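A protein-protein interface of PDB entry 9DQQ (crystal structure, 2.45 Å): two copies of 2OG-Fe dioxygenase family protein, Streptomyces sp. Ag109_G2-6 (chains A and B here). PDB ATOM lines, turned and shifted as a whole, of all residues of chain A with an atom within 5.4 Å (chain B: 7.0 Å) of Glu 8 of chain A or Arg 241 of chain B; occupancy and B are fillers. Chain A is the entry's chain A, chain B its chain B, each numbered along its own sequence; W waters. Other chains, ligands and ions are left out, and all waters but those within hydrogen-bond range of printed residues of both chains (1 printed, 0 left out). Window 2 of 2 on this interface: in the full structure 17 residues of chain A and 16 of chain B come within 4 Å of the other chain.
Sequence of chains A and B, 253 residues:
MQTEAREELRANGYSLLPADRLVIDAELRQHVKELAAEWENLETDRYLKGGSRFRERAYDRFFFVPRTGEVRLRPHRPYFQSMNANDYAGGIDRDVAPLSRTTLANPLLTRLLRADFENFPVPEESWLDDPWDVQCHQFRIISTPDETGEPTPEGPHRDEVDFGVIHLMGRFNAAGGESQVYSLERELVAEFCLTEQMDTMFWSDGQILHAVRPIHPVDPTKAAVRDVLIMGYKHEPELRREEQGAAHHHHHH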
ATOM      1  N   THR A   3     -11.540   0.230  32.724  1.00  0.00           N
ATOM      2  CA  THR A   3     -10.276   0.011  32.018  1.00  0.00           C
ATOM      3  C   THR A   3     -10.130  -1.445  31.590  1.00  0.00           C
ATOM      4  O   THR A   3      -9.779  -1.733  30.436  1.00  0.00           O
ATOM      5  CB  THR A   3      -9.094   0.422  32.899  1.00  0.00           C
ATOM      6  OG1 THR A   3      -9.297  -0.086  34.222  1.00  0.00           O
ATOM      7  CG2 THR A   3      -8.948   1.934  32.940  1.00  0.00           C
ATOM      8  N   GLU A   4     -10.381  -2.382  32.517  1.00  0.00           N
ATOM      9  CA  GLU A   4     -10.313  -3.794  32.165  1.00  0.00           C
ATOM     10  C   GLU A   4     -11.307  -4.121  31.066  1.00  0.00           C
ATOM     11  O   GLU A   4     -10.969  -4.821  30.101  1.00  0.00           O
ATOM     12  CB  GLU A   4     -10.568  -4.671  33.392  1.00  0.00           C
ATOM     13  CG  GLU A   4     -10.631  -6.186  33.093  1.00  0.00           C
ATOM     14  CD  GLU A   4      -9.273  -6.820  32.758  1.00  0.00           C
ATOM     15  OE1 GLU A   4      -8.539  -6.287  31.887  1.00  0.00           O
ATOM     16  OE2 GLU A   4      -8.938  -7.862  33.371  1.00  0.00           O
ATOM     17  N   ALA A   5     -12.533  -3.593  31.180  1.00  0.00           N
ATOM     18  CA  ALA A   5     -13.539  -3.825  30.148  1.00  0.00           C
ATOM     19  C   ALA A   5     -13.084  -3.287  28.795  1.00  0.00           C
ATOM     20  O   ALA A   5     -13.317  -3.921  27.756  1.00  0.00           O
ATOM     21  CB  ALA A   5     -14.874  -3.200  30.559  1.00  0.00           C
ATOM     22  N   ARG A   6     -12.417  -2.126  28.783  1.00  0.00           N
ATOM     23  CA  ARG A   6     -11.926  -1.572  27.522  1.00  0.00           C
ATOM     24  C   ARG A   6     -10.897  -2.495  26.874  1.00  0.00           C
ATOM     25  O   ARG A   6     -11.043  -2.893  25.713  1.00  0.00           O
ATOM     26  CB  ARG A   6     -11.339  -0.178  27.736  1.00  0.00           C
ATOM     27  CG  ARG A   6     -12.373   0.914  27.951  1.00  0.00           C
ATOM     28  CD  ARG A   6     -11.712   2.259  28.147  1.00  0.00           C
ATOM     29  NE  ARG A   6     -12.595   3.189  28.839  1.00  0.00           N
ATOM     30  CZ  ARG A   6     -12.543   4.509  28.718  1.00  0.00           C
ATOM     31  NH1 ARG A   6     -11.650   5.100  27.933  1.00  0.00           N
ATOM     32  NH2 ARG A   6     -13.417   5.257  29.391  1.00  0.00           N
ATOM     33  N   GLU A   7      -9.854  -2.863  27.620  1.00  0.00           N
ATOM     34  CA  GLU A   7      -8.843  -3.760  27.068  1.00  0.00           C
ATOM     35  C   GLU A   7      -9.455  -5.087  26.662  1.00  0.00           C
ATOM     36  O   GLU A   7      -9.167  -5.610  25.575  1.00  0.00           O
ATOM     37  CB  GLU A   7      -7.718  -3.975  28.074  1.00  0.00           C
ATOM     38  CG  GLU A   7      -6.604  -2.939  27.969  1.00  0.00           C
ATOM     39  CD  GLU A   7      -5.786  -3.082  26.689  1.00  0.00           C
ATOM     40  OE1 GLU A   7      -5.723  -4.208  26.135  1.00  0.00           O
ATOM     41  OE2 GLU A   7      -5.205  -2.066  26.239  1.00  0.00           O
ATOM     42  N   GLU A   8     -10.330  -5.633  27.517  1.00  0.00           N
ATOM     43  CA  GLU A   8     -11.052  -6.860  27.179  1.00  0.00           C
ATOM     44  C   GLU A   8     -11.800  -6.722  25.860  1.00  0.00           C
ATOM     45  O   GLU A   8     -11.798  -7.650  25.038  1.00  0.00           O
ATOM     46  CB  GLU A   8     -12.026  -7.254  28.295  1.00  0.00           C
ATOM     47  CG  GLU A   8     -11.351  -7.877  29.509  1.00  0.00           C
ATOM     48  CD  GLU A   8     -12.327  -8.512  30.480  1.00  0.00           C
ATOM     49  OE1 GLU A   8     -13.481  -8.034  30.577  1.00  0.00           O
ATOM     50  OE2 GLU A   8     -11.938  -9.487  31.156  1.00  0.00           O
ATOM     51  N   LEU A   9     -12.440  -5.570  25.627  1.00  0.00           N
ATOM     52  CA  LEU A   9     -13.098  -5.393  24.341  1.00  0.00           C
ATOM     53  C   LEU A   9     -12.074  -5.332  23.217  1.00  0.00           C
ATOM     54  O   LEU A   9     -12.324  -5.835  22.116  1.00  0.00           O
ATOM     55  CB  LEU A   9     -13.982  -4.145  24.353  1.00  0.00           C
ATOM     56  CG  LEU A   9     -15.484  -4.432  24.449  1.00  0.00           C
ATOM     57  CD1 LEU A   9     -15.729  -5.365  25.588  1.00  0.00           C
ATOM     58  CD2 LEU A   9     -16.294  -3.152  24.653  1.00  0.00           C
ATOM     59  N   ARG A  10     -10.902  -4.751  23.479  1.00  0.00           N
ATOM     60  CA  ARG A  10      -9.893  -4.644  22.426  1.00  0.00           C
ATOM     61  C   ARG A  10      -9.294  -6.005  22.094  1.00  0.00           C
ATOM     62  O   ARG A  10      -9.254  -6.407  20.926  1.00  0.00           O
ATOM     63  CB  ARG A  10      -8.812  -3.637  22.819  1.00  0.00           C
ATOM     64  CG  ARG A  10      -9.057  -2.241  22.240  1.00  0.00           C
ATOM     65  CD  ARG A  10      -7.926  -1.272  22.544  1.00  0.00           C
ATOM     66  NE  ARG A  10      -7.829  -0.975  23.972  1.00  0.00           N
ATOM     67  CZ  ARG A  10      -8.150   0.187  24.529  1.00  0.00           C
ATOM     68  NH1 ARG A  10      -8.575   1.208  23.804  1.00  0.00           N
ATOM     69  NH2 ARG A  10      -8.037   0.328  25.850  1.00  0.00           N
ATOM     70  N   ALA A  11      -8.879  -6.753  23.111  1.00  0.00           N
ATOM     71  CA  ALA A  11      -8.353  -8.097  22.875  1.00  0.00           C
ATOM     72  C   ALA A  11      -9.430  -9.051  22.346  1.00  0.00           C
ATOM     73  O   ALA A  11      -9.290  -9.626  21.259  1.00  0.00           O
ATOM     74  CB  ALA A  11      -7.736  -8.645  24.160  1.00  0.00           C
ATOM     75  N   ASN A  12     -10.527  -9.219  23.096  1.00  0.00           N
ATOM     76  CA  ASN A  12     -11.484 -10.302  22.864  1.00  0.00           C
ATOM     77  C   ASN A  12     -12.766  -9.870  22.176  1.00  0.00           C
ATOM     78  O   ASN A  12     -13.485 -10.734  21.677  1.00  0.00           O
ATOM     79  CB  ASN A  12     -11.865 -10.965  24.191  1.00  0.00           C
ATOM     80  CG  ASN A  12     -10.695 -11.071  25.149  1.00  0.00           C
ATOM     81  OD1 ASN A  12     -10.782 -10.682  26.322  1.00  0.00           O
ATOM     82  ND2 ASN A  12      -9.584 -11.597  24.650  1.00  0.00           N
ATOM     83  N   GLY A  13     -13.086  -8.574  22.153  1.00  0.00           N
ATOM     84  CA  GLY A  13     -14.301  -8.117  21.500  1.00  0.00           C
ATOM     85  C   GLY A  13     -15.553  -8.199  22.347  1.00  0.00           C
ATOM     86  O   GLY A  13     -16.645  -7.964  21.824  1.00  0.00           O
ATOM     87  N   TYR A  14     -15.430  -8.555  23.627  1.00  0.00           N
ATOM     88  CA  TYR A  14     -16.545  -8.620  24.563  1.00  0.00           C
ATOM     89  C   TYR A  14     -15.957  -8.589  25.962  1.00  0.00           C
ATOM     90  O   TYR A  14     -14.768  -8.834  26.150  1.00  0.00           O
ATOM     91  CB  TYR A  14     -17.414  -9.883  24.373  1.00  0.00           C
ATOM     92  CG  TYR A  14     -16.709 -11.157  24.809  1.00  0.00           C
ATOM     93  CD1 TYR A  14     -15.828 -11.814  23.955  1.00  0.00           C
ATOM     94  CD2 TYR A  14     -16.913 -11.689  26.077  1.00  0.00           C
ATOM     95  CE1 TYR A  14     -15.179 -12.977  24.351  1.00  0.00           C
ATOM     96  CE2 TYR A  14     -16.271 -12.853  26.483  1.00  0.00           C
ATOM     97  CZ  TYR A  14     -15.401 -13.495  25.618  1.00  0.00           C
ATOM     98  OH  TYR A  14     -14.751 -14.652  26.030  1.00  0.00           O
ATOM     99  N   SER A  15     -16.804  -8.283  26.942  1.00  0.00           N
ATOM    100  CA  SER A  15     -16.397  -8.248  28.343  1.00  0.00           C
ATOM    101  C   SER A  15     -17.610  -8.528  29.211  1.00  0.00           C
ATOM    102  O   SER A  15     -18.720  -8.105  28.884  1.00  0.00           O
ATOM    103  CB  SER A  15     -15.788  -6.898  28.726  1.00  0.00           C
ATOM    104  OG  SER A  15     -15.871  -6.681  30.117  1.00  0.00           O
ATOM    105  N   LEU A  16     -17.392  -9.218  30.323  1.00  0.00           N
ATOM    106  CA  LEU A  16     -18.475  -9.671  31.181  1.00  0.00           C
ATOM    107  C   LEU A  16     -18.437  -8.930  32.506  1.00  0.00           C
ATOM    108  O   LEU A  16     -17.368  -8.634  33.036  1.00  0.00           O
ATOM    109  CB  LEU A  16     -18.384 -11.182  31.432  1.00  0.00           C
ATOM    110  CG  LEU A  16     -18.301 -12.014  30.149  1.00  0.00           C
ATOM    111  CD1 LEU A  16     -18.129 -13.500  30.457  1.00  0.00           C
ATOM    112  CD2 LEU A  16     -19.518 -11.787  29.272  1.00  0.00           C
ATOM    113  N   PHE B  63     -11.300 -22.867  28.487  1.00  0.00           N
ATOM    114  CA  PHE B  63     -11.217 -21.773  29.437  1.00  0.00           C
ATOM    115  C   PHE B  63     -12.594 -21.566  30.062  1.00  0.00           C
ATOM    116  O   PHE B  63     -13.571 -21.356  29.342  1.00  0.00           O
ATOM    117  CB  PHE B  63     -10.754 -20.507  28.704  1.00  0.00           C
ATOM    118  CG  PHE B  63     -10.636 -19.300  29.585  1.00  0.00           C
ATOM    119  CD1 PHE B  63     -11.723 -18.456  29.789  1.00  0.00           C
ATOM    120  CD2 PHE B  63      -9.440 -19.001  30.199  1.00  0.00           C
ATOM    121  CE1 PHE B  63     -11.613 -17.343  30.602  1.00  0.00           C
ATOM    122  CE2 PHE B  63      -9.323 -17.900  31.008  1.00  0.00           C
ATOM    123  CZ  PHE B  63     -10.410 -17.062  31.204  1.00  0.00           C
ATOM    124  N   VAL B  65     -15.049 -19.913  33.399  1.00  0.00           N
ATOM    125  CA  VAL B  65     -15.253 -19.099  34.601  1.00  0.00           C
ATOM    126  C   VAL B  65     -16.652 -19.347  35.153  1.00  0.00           C
ATOM    127  O   VAL B  65     -17.656 -19.015  34.511  1.00  0.00           O
ATOM    128  CB  VAL B  65     -15.040 -17.603  34.334  1.00  0.00           C
ATOM    129  CG1 VAL B  65     -15.242 -16.822  35.627  1.00  0.00           C
ATOM    130  CG2 VAL B  65     -13.667 -17.355  33.739  1.00  0.00           C
ATOM    131  N   THR B  68     -19.611 -16.382  35.546  1.00  0.00           N
ATOM    132  CA  THR B  68     -20.228 -15.965  34.307  1.00  0.00           C
ATOM    133  C   THR B  68     -20.595 -17.129  33.401  1.00  0.00           C
ATOM    134  O   THR B  68     -21.321 -16.922  32.417  1.00  0.00           O
ATOM    135  CB  THR B  68     -19.287 -15.015  33.571  1.00  0.00           C
ATOM    136  OG1 THR B  68     -18.071 -15.704  33.279  1.00  0.00           O
ATOM    137  CG2 THR B  68     -19.000 -13.771  34.446  1.00  0.00           C
ATOM    138  N   GLU B  70     -18.543 -18.430  31.454  1.00  0.00           N
ATOM    139  CA  GLU B  70     -17.756 -18.256  30.242  1.00  0.00           C
ATOM    140  C   GLU B  70     -17.001 -19.542  29.906  1.00  0.00           C
ATOM    141  O   GLU B  70     -16.324 -20.126  30.750  1.00  0.00           O
ATOM    142  CB  GLU B  70     -16.771 -17.092  30.409  1.00  0.00           C
ATOM    143  CG  GLU B  70     -16.046 -16.712  29.117  1.00  0.00           C
ATOM    144  CD  GLU B  70     -14.964 -15.669  29.336  1.00  0.00           C
ATOM    145  OE1 GLU B  70     -14.705 -15.333  30.512  1.00  0.00           O
ATOM    146  OE2 GLU B  70     -14.371 -15.188  28.342  1.00  0.00           O
ATOM    147  N   ARG B  72     -14.463 -21.021  26.666  1.00  0.00           N
ATOM    148  CA  ARG B  72     -13.704 -20.723  25.455  1.00  0.00           C
ATOM    149  C   ARG B  72     -12.926 -21.969  25.062  1.00  0.00           C
ATOM    150  O   ARG B  72     -12.216 -22.546  25.894  1.00  0.00           O
ATOM    151  CB  ARG B  72     -12.731 -19.549  25.673  1.00  0.00           C
ATOM    152  CG  ARG B  72     -13.340 -18.230  26.147  1.00  0.00           C
ATOM    153  CD  ARG B  72     -12.266 -17.161  26.539  1.00  0.00           C
ATOM    154  NE  ARG B  72     -11.315 -16.900  25.466  1.00  0.00           N
ATOM    155  CZ  ARG B  72     -11.451 -15.976  24.523  1.00  0.00           C
ATOM    156  NH1 ARG B  72     -12.494 -15.155  24.492  1.00  0.00           N
ATOM    157  NH2 ARG B  72     -10.513 -15.871  23.584  1.00  0.00           N
ATOM    158  N   PRO B 131     -10.148 -18.085  36.539  1.00  0.00           N
ATOM    159  CA  PRO B 131     -10.239 -19.023  35.413  1.00  0.00           C
ATOM    160  C   PRO B 131     -10.012 -20.465  35.851  1.00  0.00           C
ATOM    161  O   PRO B 131      -9.367 -20.745  36.862  1.00  0.00           O
ATOM    162  CB  PRO B 131      -9.127 -18.553  34.462  1.00  0.00           C
ATOM    163  CG  PRO B 131      -8.821 -17.176  34.870  1.00  0.00           C
ATOM    164  CD  PRO B 131      -9.064 -17.113  36.345  1.00  0.00           C
ATOM    165  N   LEU B 239      -4.433 -18.201  34.397  1.00  0.00           N
ATOM    166  CA  LEU B 239      -4.670 -18.537  33.000  1.00  0.00           C
ATOM    167  C   LEU B 239      -5.267 -17.339  32.269  1.00  0.00           C
ATOM    168  O   LEU B 239      -6.072 -16.593  32.832  1.00  0.00           O
ATOM    169  CB  LEU B 239      -5.602 -19.741  32.899  1.00  0.00           C
ATOM    170  CG  LEU B 239      -6.024 -20.156  31.493  1.00  0.00           C
ATOM    171  CD1 LEU B 239      -4.825 -20.564  30.684  1.00  0.00           C
ATOM    172  CD2 LEU B 239      -7.039 -21.279  31.568  1.00  0.00           C
ATOM    173  N   ARG B 240      -4.862 -17.147  31.015  1.00  0.00           N
ATOM    174  CA  ARG B 240      -5.312 -16.021  30.208  1.00  0.00           C
ATOM    175  C   ARG B 240      -6.081 -16.517  28.991  1.00  0.00           C
ATOM    176  O   ARG B 240      -5.915 -17.656  28.542  1.00  0.00           O
ATOM    177  CB  ARG B 240      -4.135 -15.142  29.734  1.00  0.00           C
ATOM    178  CG  ARG B 240      -3.180 -14.673  30.822  1.00  0.00           C
ATOM    179  CD  ARG B 240      -2.059 -13.817  30.244  1.00  0.00           C
ATOM    180  NE  ARG B 240      -2.491 -12.455  29.937  1.00  0.00           N
ATOM    181  CZ  ARG B 240      -2.770 -12.003  28.721  1.00  0.00           C
ATOM    182  NH1 ARG B 240      -2.689 -12.784  27.656  1.00  0.00           N
ATOM    183  NH2 ARG B 240      -3.136 -10.732  28.570  1.00  0.00           N
ATOM    184  N   ARG B 241      -6.918 -15.636  28.447  1.00  0.00           N
ATOM    185  CA  ARG B 241      -7.643 -15.970  27.234  1.00  0.00           C
ATOM    186  C   ARG B 241      -6.668 -16.069  26.064  1.00  0.00           C
ATOM    187  O   ARG B 241      -5.674 -15.343  25.994  1.00  0.00           O
ATOM    188  CB  ARG B 241      -8.737 -14.929  26.976  1.00  0.00           C
ATOM    189  CG  ARG B 241      -9.654 -14.787  28.191  1.00  0.00           C
ATOM    190  CD  ARG B 241     -10.735 -13.749  28.023  1.00  0.00           C
ATOM    191  NE  ARG B 241     -11.670 -13.757  29.146  1.00  0.00           N
ATOM    192  CZ  ARG B 241     -11.439 -13.192  30.325  1.00  0.00           C
ATOM    193  NH1 ARG B 241     -10.292 -12.584  30.585  1.00  0.00           N
ATOM    194  NH2 ARG B 241     -12.379 -13.238  31.268  1.00  0.00           N
ATOM    195  N   GLU B 242      -6.951 -16.994  25.149  1.00  0.00           N
ATOM    196  CA  GLU B 242      -6.096 -17.273  24.000  1.00  0.00           C
ATOM    197  C   GLU B 242      -6.848 -17.002  22.705  1.00  0.00           C
ATOM    198  O   GLU B 242      -7.972 -17.482  22.518  1.00  0.00           O
ATOM    199  CB  GLU B 242      -5.608 -18.724  24.028  1.00  0.00           C
ATOM    200  CG  GLU B 242      -4.691 -19.029  25.204  1.00  0.00           C
ATOM    201  CD  GLU B 242      -4.585 -20.518  25.508  1.00  0.00           C
ATOM    202  OE1 GLU B 242      -5.640 -21.174  25.664  1.00  0.00           O
ATOM    203  OE2 GLU B 242      -3.448 -21.029  25.583  1.00  0.00           O
ATOM    204  N   GLU B 243      -6.214 -16.257  21.806  1.00  0.00           N
ATOM    205  CA  GLU B 243      -6.849 -15.862  20.552  1.00  0.00           C
ATOM    206  C   GLU B 243      -6.151 -16.490  19.347  1.00  0.00           C
ATOM    207  O   GLU B 243      -6.708 -17.352  18.663  1.00  0.00           O
ATOM    208  CB  GLU B 243      -6.858 -14.328  20.424  1.00  0.00           C
ATOM    209  CG  GLU B 243      -7.656 -13.573  21.509  1.00  0.00           C
ATOM    210  CD  GLU B 243      -9.173 -13.742  21.375  1.00  0.00           C
ATOM    211  OE1 GLU B 243      -9.648 -14.062  20.260  1.00  0.00           O
ATOM    212  OE2 GLU B 243      -9.899 -13.562  22.383  1.00  0.00           O
HETATM  213  O   HOH W   1     -12.713 -13.033  21.868  1.00  0.00           O
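Asn 12 of chain A touches Arg 241 of chain B (OD1 to CD, 3.5 Å).
CD1 of Leu 16 of chain A touches OG1 of Thr 68 of chain B, at 3.6 Å.
Glu 70 of chain B touches Leu 16 of chain A.
No position is printed for both chains.
The backbone carbonyl oxygen (O) of Glu 242 of chain B is in hydrogen-bond range of the guanidinium group (NH2) of Arg 72 of chain B (3.2 Å).
O of Glu 8 of chain A lies within hydrogen-bond range of N of Gly 13 of chain A, 3.3 Å away.
OG of Ser 15 of chain A is in hydrogen-bond range of OE1 of Glu 8 of chain A, at 2.8 Å.
The side-chain carboxylate (OE2) of Glu 243 of chain B lies within salt-bridge range of the guanidinium group (NH2) of Arg 72 of chain B (2.7 Å).
O of Glu 8 of chain A sits close to OD1 of Asn 12 of chain A, 3.4 Å away.
O of Glu 70 of chain B is in hydrogen-bond range of N of Val 65 of chain B, 2.9 Å away.
OH of Tyr 14 of chain A sits at hydrogen-bond distance from OE2 of Glu 70 of chain B, 2.4 Å away.
The guanidinium group (NH1) of Arg 241 of chain B is in salt-bridge range of the side-chain carboxylate (OE2) of Glu 8 of chain A.
The side-chain amide nitrogen of Asn 12 of chain A is in hydrogen-bond range of the side-chain carboxylate of Glu 243 of chain B (3.0 Å).
The guanidinium group of Arg 72 of chain B lies within hydrogen-bond range of the side-chain hydroxyl of Tyr 14 of chain A, at 2.8 Å.
Water W1 lies within hydrogen-bond range of the backbone carbonyl oxygen of Asn 12 of chain A (2.4 Å), the side-chain carboxylate of Glu 243 of chain B (2.9 Å) and the guanidinium group of Arg 72 of chain B (3.4 Å).
Of the 14 printed residues of chain A, 4 touch a printed residue of chain B.
Hydrophobic or aromatic side chains of chain A within 4 Å of the printed part of chain B: Tyr 14 and Leu 16.
Of the 11 printed residues of chain B, 5 touch a printed residue of chain A.
Glu 8 of chain A touches just one residue of chain B: Arg 241 (3.6 Å).
Arg 241 of chain B touches two residues of chain A.
Of the printed residues of chain B, Asn 12 of chain A touches Arg 241 and Glu 243.
Printed residues of chain A within 4 Å of Thr 68 of chain B: Leu 16.
The nearest residue of chain A that does not touch Arg 241 of chain B is Tyr 14 of chain A (4.5 Å).
The nearest printed residue of chain A that does not touch Arg 72 of chain B is Asn 12 of chain A (4.2 Å).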
